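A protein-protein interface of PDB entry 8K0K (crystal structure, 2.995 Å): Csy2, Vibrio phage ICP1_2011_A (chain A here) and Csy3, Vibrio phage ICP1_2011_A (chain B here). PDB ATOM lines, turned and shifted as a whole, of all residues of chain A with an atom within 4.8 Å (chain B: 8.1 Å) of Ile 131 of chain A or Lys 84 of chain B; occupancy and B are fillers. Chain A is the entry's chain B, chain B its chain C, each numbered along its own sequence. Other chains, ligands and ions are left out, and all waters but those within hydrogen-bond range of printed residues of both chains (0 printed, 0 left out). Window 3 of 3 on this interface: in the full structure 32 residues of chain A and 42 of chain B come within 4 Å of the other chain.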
ATOM      1  N   VAL A  10      10.112  29.418 -15.688  1.00  0.00           N
ATOM      2  CA  VAL A  10       9.418  29.567 -16.965  1.00  0.00           C
ATOM      3  C   VAL A  10      10.505  29.824 -18.006  1.00  0.00           C
ATOM      4  O   VAL A  10      10.949  30.954 -18.207  1.00  0.00           O
ATOM      5  CB  VAL A  10       8.375  30.678 -16.923  1.00  0.00           C
ATOM      6  CG1 VAL A  10       7.486  30.623 -18.155  1.00  0.00           C
ATOM      7  CG2 VAL A  10       7.550  30.581 -15.654  1.00  0.00           C
ATOM      8  N   LYS A  11      10.956  28.755 -18.660  1.00  0.00           N
ATOM      9  CA  LYS A  11      11.904  28.891 -19.759  1.00  0.00           C
ATOM     10  C   LYS A  11      11.187  29.477 -20.970  1.00  0.00           C
ATOM     11  O   LYS A  11      10.221  28.893 -21.471  1.00  0.00           O
ATOM     12  CB  LYS A  11      12.524  27.536 -20.101  1.00  0.00           C
ATOM     13  CG  LYS A  11      13.202  26.830 -18.930  1.00  0.00           C
ATOM     14  CD  LYS A  11      13.955  25.588 -19.399  1.00  0.00           C
ATOM     15  CE  LYS A  11      14.424  24.730 -18.230  1.00  0.00           C
ATOM     16  NZ  LYS A  11      15.329  25.472 -17.309  1.00  0.00           N
ATOM     17  N   VAL A  12      11.645  30.637 -21.436  1.00  0.00           N
ATOM     18  CA  VAL A  12      11.022  31.335 -22.554  1.00  0.00           C
ATOM     19  C   VAL A  12      12.083  31.612 -23.607  1.00  0.00           C
ATOM     20  O   VAL A  12      13.153  32.144 -23.292  1.00  0.00           O
ATOM     21  CB  VAL A  12      10.350  32.646 -22.109  1.00  0.00           C
ATOM     22  CG1 VAL A  12       9.710  33.334 -23.300  1.00  0.00           C
ATOM     23  CG2 VAL A  12       9.320  32.363 -21.029  1.00  0.00           C
ATOM     24  N   ILE A 121      -1.614  29.352 -19.278  1.00  0.00           N
ATOM     25  CA  ILE A 121      -0.207  29.531 -19.640  1.00  0.00           C
ATOM     26  C   ILE A 121       0.117  28.762 -20.912  1.00  0.00           C
ATOM     27  O   ILE A 121       0.840  29.254 -21.787  1.00  0.00           O
ATOM     28  CB  ILE A 121       0.712  29.109 -18.476  1.00  0.00           C
ATOM     29  CG1 ILE A 121       0.634  30.115 -17.327  1.00  0.00           C
ATOM     30  CG2 ILE A 121       2.149  28.988 -18.946  1.00  0.00           C
ATOM     31  CD1 ILE A 121       1.635  29.845 -16.217  1.00  0.00           C
ATOM     32  N   ASN A 122      -0.444  27.559 -21.053  1.00  0.00           N
ATOM     33  CA  ASN A 122      -0.210  26.757 -22.250  1.00  0.00           C
ATOM     34  C   ASN A 122      -0.635  27.454 -23.538  1.00  0.00           C
ATOM     35  O   ASN A 122      -0.228  27.011 -24.618  1.00  0.00           O
ATOM     36  CB  ASN A 122      -0.939  25.421 -22.132  1.00  0.00           C
ATOM     37  CG  ASN A 122      -0.361  24.539 -21.046  1.00  0.00           C
ATOM     38  OD1 ASN A 122       0.799  24.691 -20.664  1.00  0.00           O
ATOM     39  ND2 ASN A 122      -1.165  23.608 -20.544  1.00  0.00           N
ATOM     40  N   ALA A 124      -0.295  30.971 -23.908  1.00  0.00           N
ATOM     41  CA  ALA A 124       0.251  32.316 -23.841  1.00  0.00           C
ATOM     42  C   ALA A 124       1.691  32.353 -24.336  1.00  0.00           C
ATOM     43  O   ALA A 124       2.326  31.325 -24.593  1.00  0.00           O
ATOM     44  CB  ALA A 124       0.175  32.856 -22.408  1.00  0.00           C
ATOM     45  N   ARG A 125       2.187  33.574 -24.478  1.00  0.00           N
ATOM     46  CA  ARG A 125       3.601  33.881 -24.622  1.00  0.00           C
ATOM     47  C   ARG A 125       4.012  34.809 -23.484  1.00  0.00           C
ATOM     48  O   ARG A 125       3.203  35.172 -22.624  1.00  0.00           O
ATOM     49  CB  ARG A 125       3.894  34.516 -25.986  1.00  0.00           C
ATOM     50  CG  ARG A 125       4.053  33.522 -27.121  1.00  0.00           C
ATOM     51  CD  ARG A 125       2.955  33.681 -28.142  1.00  0.00           C
ATOM     52  NE  ARG A 125       3.412  34.338 -29.361  1.00  0.00           N
ATOM     53  CZ  ARG A 125       3.411  33.765 -30.560  1.00  0.00           C
ATOM     54  NH1 ARG A 125       2.975  32.520 -30.702  1.00  0.00           N
ATOM     55  NH2 ARG A 125       3.838  34.434 -31.622  1.00  0.00           N
ATOM     56  N   ILE A 126       5.285  35.195 -23.475  1.00  0.00           N
ATOM     57  CA  ILE A 126       5.792  36.211 -22.559  1.00  0.00           C
ATOM     58  C   ILE A 126       6.644  37.165 -23.381  1.00  0.00           C
ATOM     59  O   ILE A 126       7.701  36.775 -23.892  1.00  0.00           O
ATOM     60  CB  ILE A 126       6.602  35.617 -21.402  1.00  0.00           C
ATOM     61  CG1 ILE A 126       5.697  34.796 -20.482  1.00  0.00           C
ATOM     62  CG2 ILE A 126       7.284  36.724 -20.619  1.00  0.00           C
ATOM     63  CD1 ILE A 126       6.402  34.276 -19.247  1.00  0.00           C
ATOM     64  N   GLY A 129       7.716  35.839 -26.516  1.00  0.00           N
ATOM     65  CA  GLY A 129       8.539  34.641 -26.526  1.00  0.00           C
ATOM     66  C   GLY A 129       7.733  33.374 -26.281  1.00  0.00           C
ATOM     67  O   GLY A 129       6.847  33.326 -25.427  1.00  0.00           O
ATOM     68  N   THR A 130       8.060  32.337 -27.047  1.00  0.00           N
ATOM     69  CA  THR A 130       7.443  31.030 -26.862  1.00  0.00           C
ATOM     70  C   THR A 130       7.810  30.457 -25.497  1.00  0.00           C
ATOM     71  O   THR A 130       8.985  30.417 -25.125  1.00  0.00           O
ATOM     72  CB  THR A 130       7.894  30.083 -27.977  1.00  0.00           C
ATOM     73  OG1 THR A 130       7.213  30.413 -29.195  1.00  0.00           O
ATOM     74  CG2 THR A 130       7.613  28.633 -27.614  1.00  0.00           C
ATOM     75  N   ILE A 131       6.800  30.025 -24.745  1.00  0.00           N
ATOM     76  CA  ILE A 131       7.034  29.396 -23.447  1.00  0.00           C
ATOM     77  C   ILE A 131       7.353  27.923 -23.676  1.00  0.00           C
ATOM     78  O   ILE A 131       6.524  27.169 -24.196  1.00  0.00           O
ATOM     79  CB  ILE A 131       5.827  29.568 -22.515  1.00  0.00           C
ATOM     80  CG1 ILE A 131       5.481  31.052 -22.354  1.00  0.00           C
ATOM     81  CG2 ILE A 131       6.117  28.943 -21.159  1.00  0.00           C
ATOM     82  CD1 ILE A 131       4.284  31.326 -21.457  1.00  0.00           C
ATOM     83  N   ALA A 132       8.561  27.514 -23.292  1.00  0.00           N
ATOM     84  CA  ALA A 132       9.033  26.162 -23.559  1.00  0.00           C
ATOM     85  C   ALA A 132       8.676  25.186 -22.447  1.00  0.00           C
ATOM     86  O   ALA A 132       8.338  24.032 -22.728  1.00  0.00           O
ATOM     87  CB  ALA A 132      10.549  26.166 -23.770  1.00  0.00           C
ATOM     88  N   SER A 133       8.745  25.624 -21.192  1.00  0.00           N
ATOM     89  CA  SER A 133       8.512  24.733 -20.064  1.00  0.00           C
ATOM     90  C   SER A 133       8.382  25.557 -18.791  1.00  0.00           C
ATOM     91  O   SER A 133       9.090  26.550 -18.612  1.00  0.00           O
ATOM     92  CB  SER A 133       9.651  23.714 -19.911  1.00  0.00           C
ATOM     93  OG  SER A 133      10.775  24.293 -19.274  1.00  0.00           O
ATOM     94  N   PHE A 134       7.484  25.132 -17.909  1.00  0.00           N
ATOM     95  CA  PHE A 134       7.331  25.762 -16.608  1.00  0.00           C
ATOM     96  C   PHE A 134       7.051  24.684 -15.574  1.00  0.00           C
ATOM     97  O   PHE A 134       6.541  23.608 -15.902  1.00  0.00           O
ATOM     98  CB  PHE A 134       6.208  26.816 -16.607  1.00  0.00           C
ATOM     99  CG  PHE A 134       4.881  26.299 -17.095  1.00  0.00           C
ATOM    100  CD1 PHE A 134       4.622  26.185 -18.451  1.00  0.00           C
ATOM    101  CD2 PHE A 134       3.885  25.945 -16.200  1.00  0.00           C
ATOM    102  CE1 PHE A 134       3.406  25.714 -18.905  1.00  0.00           C
ATOM    103  CE2 PHE A 134       2.665  25.474 -16.649  1.00  0.00           C
ATOM    104  CZ  PHE A 134       2.427  25.360 -18.004  1.00  0.00           C
ATOM    105  N   ARG B  14       1.663  32.716 -35.562  1.00  0.00           N
ATOM    106  CA  ARG B  14       2.167  31.412 -35.961  1.00  0.00           C
ATOM    107  C   ARG B  14       1.507  30.318 -35.126  1.00  0.00           C
ATOM    108  O   ARG B  14       1.142  30.522 -33.962  1.00  0.00           O
ATOM    109  CB  ARG B  14       3.692  31.349 -35.819  1.00  0.00           C
ATOM    110  CG  ARG B  14       4.186  30.894 -34.447  1.00  0.00           C
ATOM    111  CD  ARG B  14       5.698  30.710 -34.408  1.00  0.00           C
ATOM    112  NE  ARG B  14       6.411  31.983 -34.460  1.00  0.00           N
ATOM    113  CZ  ARG B  14       6.685  32.730 -33.394  1.00  0.00           C
ATOM    114  NH1 ARG B  14       6.302  32.335 -32.186  1.00  0.00           N
ATOM    115  NH2 ARG B  14       7.341  33.875 -33.536  1.00  0.00           N
ATOM    116  N   LYS B  15       1.334  29.148 -35.742  1.00  0.00           N
ATOM    117  CA  LYS B  15       0.685  28.023 -35.088  1.00  0.00           C
ATOM    118  C   LYS B  15       1.615  26.847 -34.834  1.00  0.00           C
ATOM    119  O   LYS B  15       1.267  25.967 -34.042  1.00  0.00           O
ATOM    120  CB  LYS B  15      -0.516  27.553 -35.920  1.00  0.00           C
ATOM    121  CG  LYS B  15      -1.528  28.657 -36.188  1.00  0.00           C
ATOM    122  CD  LYS B  15      -1.978  29.313 -34.889  1.00  0.00           C
ATOM    123  CE  LYS B  15      -2.872  30.514 -35.154  1.00  0.00           C
ATOM    124  NZ  LYS B  15      -3.391  31.094 -33.884  1.00  0.00           N
ATOM    125  N   ILE B  16       2.773  26.809 -35.484  1.00  0.00           N
ATOM    126  CA  ILE B  16       3.837  25.864 -35.164  1.00  0.00           C
ATOM    127  C   ILE B  16       4.879  26.630 -34.360  1.00  0.00           C
ATOM    128  O   ILE B  16       5.624  27.445 -34.915  1.00  0.00           O
ATOM    129  CB  ILE B  16       4.453  25.253 -36.428  1.00  0.00           C
ATOM    130  CG1 ILE B  16       3.358  24.759 -37.373  1.00  0.00           C
ATOM    131  CG2 ILE B  16       5.408  24.122 -36.061  1.00  0.00           C
ATOM    132  CD1 ILE B  16       3.888  24.256 -38.697  1.00  0.00           C
ATOM    133  N   ASN B  17       4.939  26.380 -33.051  1.00  0.00           N
ATOM    134  CA  ASN B  17       5.804  27.127 -32.145  1.00  0.00           C
ATOM    135  C   ASN B  17       6.890  26.209 -31.600  1.00  0.00           C
ATOM    136  O   ASN B  17       6.670  25.491 -30.612  1.00  0.00           O
ATOM    137  CB  ASN B  17       4.982  27.737 -31.007  1.00  0.00           C
ATOM    138  CG  ASN B  17       4.058  28.842 -31.488  1.00  0.00           C
ATOM    139  OD1 ASN B  17       4.269  30.017 -31.186  1.00  0.00           O
ATOM    140  ND2 ASN B  17       3.038  28.471 -32.253  1.00  0.00           N
ATOM    141  N   PRO B  18       8.061  26.160 -32.227  1.00  0.00           N
ATOM    142  CA  PRO B  18       9.169  25.382 -31.676  1.00  0.00           C
ATOM    143  C   PRO B  18       9.979  26.195 -30.678  1.00  0.00           C
ATOM    144  O   PRO B  18       9.970  27.427 -30.677  1.00  0.00           O
ATOM    145  CB  PRO B  18      10.004  25.052 -32.920  1.00  0.00           C
ATOM    146  CG  PRO B  18       9.779  26.219 -33.808  1.00  0.00           C
ATOM    147  CD  PRO B  18       8.363  26.665 -33.577  1.00  0.00           C
ATOM    148  N   THR B  19      10.675  25.473 -29.809  1.00  0.00           N
ATOM    149  CA  THR B  19      11.590  26.096 -28.872  1.00  0.00           C
ATOM    150  C   THR B  19      12.996  26.090 -29.461  1.00  0.00           C
ATOM    151  O   THR B  19      13.223  25.667 -30.597  1.00  0.00           O
ATOM    152  CB  THR B  19      11.567  25.373 -27.527  1.00  0.00           C
ATOM    153  OG1 THR B  19      12.376  24.195 -27.607  1.00  0.00           O
ATOM    154  CG2 THR B  19      10.150  24.974 -27.167  1.00  0.00           C
ATOM    155  N   TYR B  81      14.441  19.526 -28.344  1.00  0.00           N
ATOM    156  CA  TYR B  81      13.545  20.680 -28.367  1.00  0.00           C
ATOM    157  C   TYR B  81      12.104  20.201 -28.227  1.00  0.00           C
ATOM    158  O   TYR B  81      11.833  19.004 -28.108  1.00  0.00           O
ATOM    159  CB  TYR B  81      13.735  21.525 -29.632  1.00  0.00           C
ATOM    160  CG  TYR B  81      13.539  20.791 -30.934  1.00  0.00           C
ATOM    161  CD1 TYR B  81      14.588  20.113 -31.532  1.00  0.00           C
ATOM    162  CD2 TYR B  81      12.313  20.801 -31.580  1.00  0.00           C
ATOM    163  CE1 TYR B  81      14.418  19.449 -32.729  1.00  0.00           C
ATOM    164  CE2 TYR B  81      12.135  20.140 -32.780  1.00  0.00           C
ATOM    165  CZ  TYR B  81      13.191  19.466 -33.348  1.00  0.00           C
ATOM    166  OH  TYR B  81      13.022  18.807 -34.541  1.00  0.00           O
ATOM    167  N   ASN B  82      11.178  21.163 -28.203  1.00  0.00           N
ATOM    168  CA  ASN B  82       9.747  20.902 -28.155  1.00  0.00           C
ATOM    169  C   ASN B  82       9.055  21.717 -29.238  1.00  0.00           C
ATOM    170  O   ASN B  82       9.548  22.770 -29.651  1.00  0.00           O
ATOM    171  CB  ASN B  82       9.133  21.257 -26.788  1.00  0.00           C
ATOM    172  CG  ASN B  82       9.628  20.362 -25.665  1.00  0.00           C
ATOM    173  OD1 ASN B  82      10.221  19.312 -25.902  1.00  0.00           O
ATOM    174  ND2 ASN B  82       9.370  20.772 -24.428  1.00  0.00           N
ATOM    175  N   VAL B  83       7.908  21.225 -29.698  1.00  0.00           N
ATOM    176  CA  VAL B  83       7.095  21.916 -30.696  1.00  0.00           C
ATOM    177  C   VAL B  83       5.651  21.923 -30.212  1.00  0.00           C
ATOM    178  O   VAL B  83       5.086  20.860 -29.931  1.00  0.00           O
ATOM    179  CB  VAL B  83       7.190  21.258 -32.082  1.00  0.00           C
ATOM    180  CG1 VAL B  83       6.348  22.028 -33.080  1.00  0.00           C
ATOM    181  CG2 VAL B  83       8.631  21.181 -32.547  1.00  0.00           C
ATOM    182  N   LYS B  84       5.051  23.110 -30.122  1.00  0.00           N
ATOM    183  CA  LYS B  84       3.650  23.256 -29.748  1.00  0.00           C
ATOM    184  C   LYS B  84       2.840  23.629 -30.984  1.00  0.00           C
ATOM    185  O   LYS B  84       3.116  24.648 -31.626  1.00  0.00           O
ATOM    186  CB  LYS B  84       3.479  24.314 -28.657  1.00  0.00           C
ATOM    187  CG  LYS B  84       2.041  24.501 -28.190  1.00  0.00           C
ATOM    188  CD  LYS B  84       1.905  25.707 -27.270  1.00  0.00           C
ATOM    189  CE  LYS B  84       2.807  25.582 -26.049  1.00  0.00           C
ATOM    190  NZ  LYS B  84       2.767  26.799 -25.182  1.00  0.00           N
ATOM    191  N   PHE B  85       1.856  22.803 -31.323  1.00  0.00           N
ATOM    192  CA  PHE B  85       0.899  23.107 -32.375  1.00  0.00           C
ATOM    193  C   PHE B  85      -0.373  23.661 -31.748  1.00  0.00           C
ATOM    194  O   PHE B  85      -0.839  23.155 -30.721  1.00  0.00           O
ATOM    195  CB  PHE B  85       0.578  21.865 -33.204  1.00  0.00           C
ATOM    196  CG  PHE B  85       1.725  21.375 -34.040  1.00  0.00           C
ATOM    197  CD1 PHE B  85       2.679  20.530 -33.501  1.00  0.00           C
ATOM    198  CD2 PHE B  85       1.839  21.750 -35.368  1.00  0.00           C
ATOM    199  CE1 PHE B  85       3.729  20.072 -34.270  1.00  0.00           C
ATOM    200  CE2 PHE B  85       2.888  21.295 -36.144  1.00  0.00           C
ATOM    201  CZ  PHE B  85       3.836  20.455 -35.593  1.00  0.00           C
ATOM    202  N   VAL B  86      -0.933  24.695 -32.380  1.00  0.00           N
ATOM    203  CA  VAL B  86      -2.042  25.470 -31.836  1.00  0.00           C
ATOM    204  C   VAL B  86      -3.156  25.546 -32.872  1.00  0.00           C
ATOM    205  O   VAL B  86      -2.902  25.593 -34.079  1.00  0.00           O
ATOM    206  CB  VAL B  86      -1.572  26.885 -31.413  1.00  0.00           C
ATOM    207  CG1 VAL B  86      -2.749  27.807 -31.098  1.00  0.00           C
ATOM    208  CG2 VAL B  86      -0.634  26.790 -30.218  1.00  0.00           C
ATOM    209  N   GLY B  87      -4.401  25.540 -32.394  1.00  0.00           N
ATOM    210  CA  GLY B  87      -5.567  25.619 -33.250  1.00  0.00           C
ATOM    211  C   GLY B  87      -5.983  27.044 -33.555  1.00  0.00           C
ATOM    212  O   GLY B  87      -5.201  27.990 -33.431  1.00  0.00           O
ATOM    213  N   ILE B 123       9.567  16.858 -38.897  1.00  0.00           N
ATOM    214  CA  ILE B 123      10.103  16.732 -37.542  1.00  0.00           C
ATOM    215  C   ILE B 123      10.765  15.371 -37.342  1.00  0.00           C
ATOM    216  O   ILE B 123      11.858  15.276 -36.769  1.00  0.00           O
ATOM    217  CB  ILE B 123       9.008  16.974 -36.489  1.00  0.00           C
ATOM    218  CG1 ILE B 123       8.508  18.415 -36.551  1.00  0.00           C
ATOM    219  CG2 ILE B 123       9.536  16.661 -35.093  1.00  0.00           C
ATOM    220  CD1 ILE B 123       7.533  18.762 -35.440  1.00  0.00           C
ATOM    221  N   VAL B 173      -2.208  16.008 -34.587  1.00  0.00           N
ATOM    222  CA  VAL B 173      -1.790  17.337 -35.030  1.00  0.00           C
ATOM    223  C   VAL B 173      -2.853  17.969 -35.927  1.00  0.00           C
ATOM    224  O   VAL B 173      -3.208  19.142 -35.761  1.00  0.00           O
ATOM    225  CB  VAL B 173      -0.418  17.272 -35.719  1.00  0.00           C
ATOM    226  CG1 VAL B 173      -0.094  18.606 -36.381  1.00  0.00           C
ATOM    227  CG2 VAL B 173       0.651  16.921 -34.696  1.00  0.00           C
ATOM    228  N   VAL B 176      -5.846  19.061 -33.890  1.00  0.00           N
ATOM    229  CA  VAL B 176      -5.689  20.354 -33.229  1.00  0.00           C
ATOM    230  C   VAL B 176      -5.743  21.493 -34.245  1.00  0.00           C
ATOM    231  O   VAL B 176      -6.398  22.516 -34.012  1.00  0.00           O
ATOM    232  CB  VAL B 176      -4.389  20.383 -32.410  1.00  0.00           C
ATOM    233  CG1 VAL B 176      -4.066  21.805 -31.994  1.00  0.00           C
ATOM    234  CG2 VAL B 176      -4.525  19.494 -31.188  1.00  0.00           C
ATOM    235  N   LEU B 177      -5.061  21.339 -35.383  1.00  0.00           N
ATOM    236  CA  LEU B 177      -5.050  22.400 -36.388  1.00  0.00           C
ATOM    237  C   LEU B 177      -6.439  22.628 -36.978  1.00  0.00           C
ATOM    238  O   LEU B 177      -6.852  23.777 -37.181  1.00  0.00           O
ATOM    239  CB  LEU B 177      -4.049  22.067 -37.496  1.00  0.00           C
ATOM    240  CG  LEU B 177      -2.563  22.252 -37.180  1.00  0.00           C
ATOM    241  CD1 LEU B 177      -1.702  21.656 -38.279  1.00  0.00           C
ATOM    242  CD2 LEU B 177      -2.238  23.723 -36.999  1.00  0.00           C
ATOM    243  N   GLY B 181      -7.512  24.063 -29.417  1.00  0.00           N
ATOM    244  CA  GLY B 181      -6.650  23.367 -28.485  1.00  0.00           C
ATOM    245  C   GLY B 181      -5.195  23.425 -28.907  1.00  0.00           C
ATOM    246  O   GLY B 181      -4.784  24.244 -29.734  1.00  0.00           O
ATOM    247  N   PHE B 182      -4.403  22.527 -28.325  1.00  0.00           N
ATOM    248  CA  PHE B 182      -2.986  22.472 -28.652  1.00  0.00           C
ATOM    249  C   PHE B 182      -2.445  21.072 -28.398  1.00  0.00           C
ATOM    250  O   PHE B 182      -3.060  20.260 -27.703  1.00  0.00           O
ATOM    251  CB  PHE B 182      -2.183  23.507 -27.854  1.00  0.00           C
ATOM    252  CG  PHE B 182      -1.983  23.143 -26.411  1.00  0.00           C
ATOM    253  CD1 PHE B 182      -0.865  22.427 -26.009  1.00  0.00           C
ATOM    254  CD2 PHE B 182      -2.903  23.529 -25.455  1.00  0.00           C
ATOM    255  CE1 PHE B 182      -0.677  22.097 -24.688  1.00  0.00           C
ATOM    256  CE2 PHE B 182      -2.719  23.201 -24.128  1.00  0.00           C
ATOM    257  CZ  PHE B 182      -1.603  22.483 -23.746  1.00  0.00           C
ATOM    258  N   VAL B 183      -1.271  20.808 -28.965  1.00  0.00           N
ATOM    259  CA  VAL B 183      -0.559  19.549 -28.736  1.00  0.00           C
ATOM    260  C   VAL B 183       0.944  19.808 -28.801  1.00  0.00           C
ATOM    261  O   VAL B 183       1.433  20.458 -29.729  1.00  0.00           O
ATOM    262  CB  VAL B 183      -0.978  18.458 -29.743  1.00  0.00           C
ATOM    263  CG1 VAL B 183      -0.870  18.963 -31.171  1.00  0.00           C
ATOM    264  CG2 VAL B 183      -0.136  17.208 -29.551  1.00  0.00           C
ATOM    265  N   THR B 184       1.678  19.295 -27.817  1.00  0.00           N
ATOM    266  CA  THR B 184       3.116  19.516 -27.712  1.00  0.00           C
ATOM    267  C   THR B 184       3.856  18.202 -27.931  1.00  0.00           C
ATOM    268  O   THR B 184       3.634  17.229 -27.200  1.00  0.00           O
ATOM    269  CB  THR B 184       3.479  20.108 -26.350  1.00  0.00           C
ATOM    270  OG1 THR B 184       2.826  21.373 -26.185  1.00  0.00           O
ATOM    271  CG2 THR B 184       4.985  20.298 -26.238  1.00  0.00           C
ATOM    272  N   LEU B 185       4.735  18.179 -28.931  1.00  0.00           N
ATOM    273  CA  LEU B 185       5.661  17.074 -29.146  1.00  0.00           C
ATOM    274  C   LEU B 185       7.006  17.419 -28.517  1.00  0.00           C
ATOM    275  O   LEU B 185       7.530  18.517 -28.733  1.00  0.00           O
ATOM    276  CB  LEU B 185       5.857  16.781 -30.637  1.00  0.00           C
ATOM    277  CG  LEU B 185       4.738  17.004 -31.656  1.00  0.00           C
ATOM    278  CD1 LEU B 185       5.202  16.557 -33.035  1.00  0.00           C
ATOM    279  CD2 LEU B 185       3.476  16.273 -31.263  1.00  0.00           C
ATOM    280  N   LYS B 186       7.563  16.487 -27.744  1.00  0.00           N
ATOM    281  CA  LYS B 186       8.900  16.624 -27.178  1.00  0.00           C
ATOM    282  C   LYS B 186       9.841  15.778 -28.025  1.00  0.00           C
ATOM    283  O   LYS B 186       9.731  14.547 -28.044  1.00  0.00           O
ATOM    284  CB  LYS B 186       8.920  16.192 -25.714  1.00  0.00           C
ATOM    285  CG  LYS B 186       7.794  16.796 -24.887  1.00  0.00           C
ATOM    286  CD  LYS B 186       8.099  16.758 -23.397  1.00  0.00           C
ATOM    287  CE  LYS B 186       9.239  17.710 -23.038  1.00  0.00           C
ATOM    288  NZ  LYS B 186       9.463  17.796 -21.566  1.00  0.00           N
ATOM    289  N   ILE B 233      10.642  23.053 -40.251  1.00  0.00           N
ATOM    290  CA  ILE B 233       9.407  22.277 -40.147  1.00  0.00           C
ATOM    291  C   ILE B 233       8.450  22.617 -41.287  1.00  0.00           C
ATOM    292  O   ILE B 233       7.925  21.725 -41.963  1.00  0.00           O
ATOM    293  CB  ILE B 233       8.746  22.496 -38.777  1.00  0.00           C
ATOM    294  CG1 ILE B 233       9.609  21.902 -37.669  1.00  0.00           C
ATOM    295  CG2 ILE B 233       7.363  21.878 -38.757  1.00  0.00           C
ATOM    296  CD1 ILE B 233       9.014  22.063 -36.282  1.00  0.00           C
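NZ of Lys 84 of chain B is in hydrogen-bond range of O of Asn 122 of chain A (3.1 Å). The side-chain amide oxygen (OD1) of Asn 17 of chain B is in hydrogen-bond range of the guanidinium group (NH1) of Arg 125 of chain A (2.9 Å). NH2 of Arg 125 of chain A sits close to NH1 of Arg 14 of chain B (3.3 Å).
The backbone carbonyl oxygen (O) of Lys 11 of chain A is in hydrogen-bond range of the backbone NH (N) of Ala 132 of chain A, 2.8 Å away. OD1 of Asn 17 of chain B sits at hydrogen-bond distance from NH1 of Arg 14 of chain B (3.2 Å). N of Asn 17 of chain B sits at hydrogen-bond distance from O of Lys 84 of chain B (2.9 Å). The backbone NH (N) of Thr 19 of chain B sits at hydrogen-bond distance from the backbone carbonyl oxygen (O) of Asn 82 of chain B.
Asn 122 of chain A touches Phe 182 of chain B. Thr 130 of chain A touches Arg 14 of chain B. Asn 17 of chain B touches Thr 130 of chain A. O of Ile 131 of chain A touches NZ of Lys 84 of chain B, 3.9 Å away. Ala 132 of chain A touches Thr 19 of chain B. Ala 132 of chain A touches Asn 82 of chain B.
Of chain B, only Lys 84 comes within 4 Å of Ile 131 of chain A. Ala 132 of chain A touches just these residues of chain B: Thr 19 and Asn 82. Printed residues of chain A within 4 Å of Arg 14 of chain B: Arg 125 (3.3 Å) and Thr 130 (3.7 Å). Of the printed residues of chain A, Asn 82 of chain B touches Ala 132 (3.8 Å). Lys 84 of chain B touches just these residues of chain A: Asn 122 (3.1 Å) and Ile 131 (3.9 Å).
Of the 24 printed residues of chain B, 6 touch a printed residue of chain A. Hydrophobic or aromatic side chains of chain B that line the printed part of chain A: Phe 182. Printed residues of chain A that touch a printed residue of chain B: Asn 122, Arg 125, Thr 130, Ile 131 and Ala 132. Hydrophobic or aromatic side chains of chain A within 4 Å of the printed part of chain B: Ala 132. Among the printed residues, 9 pairs touch across the chains.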
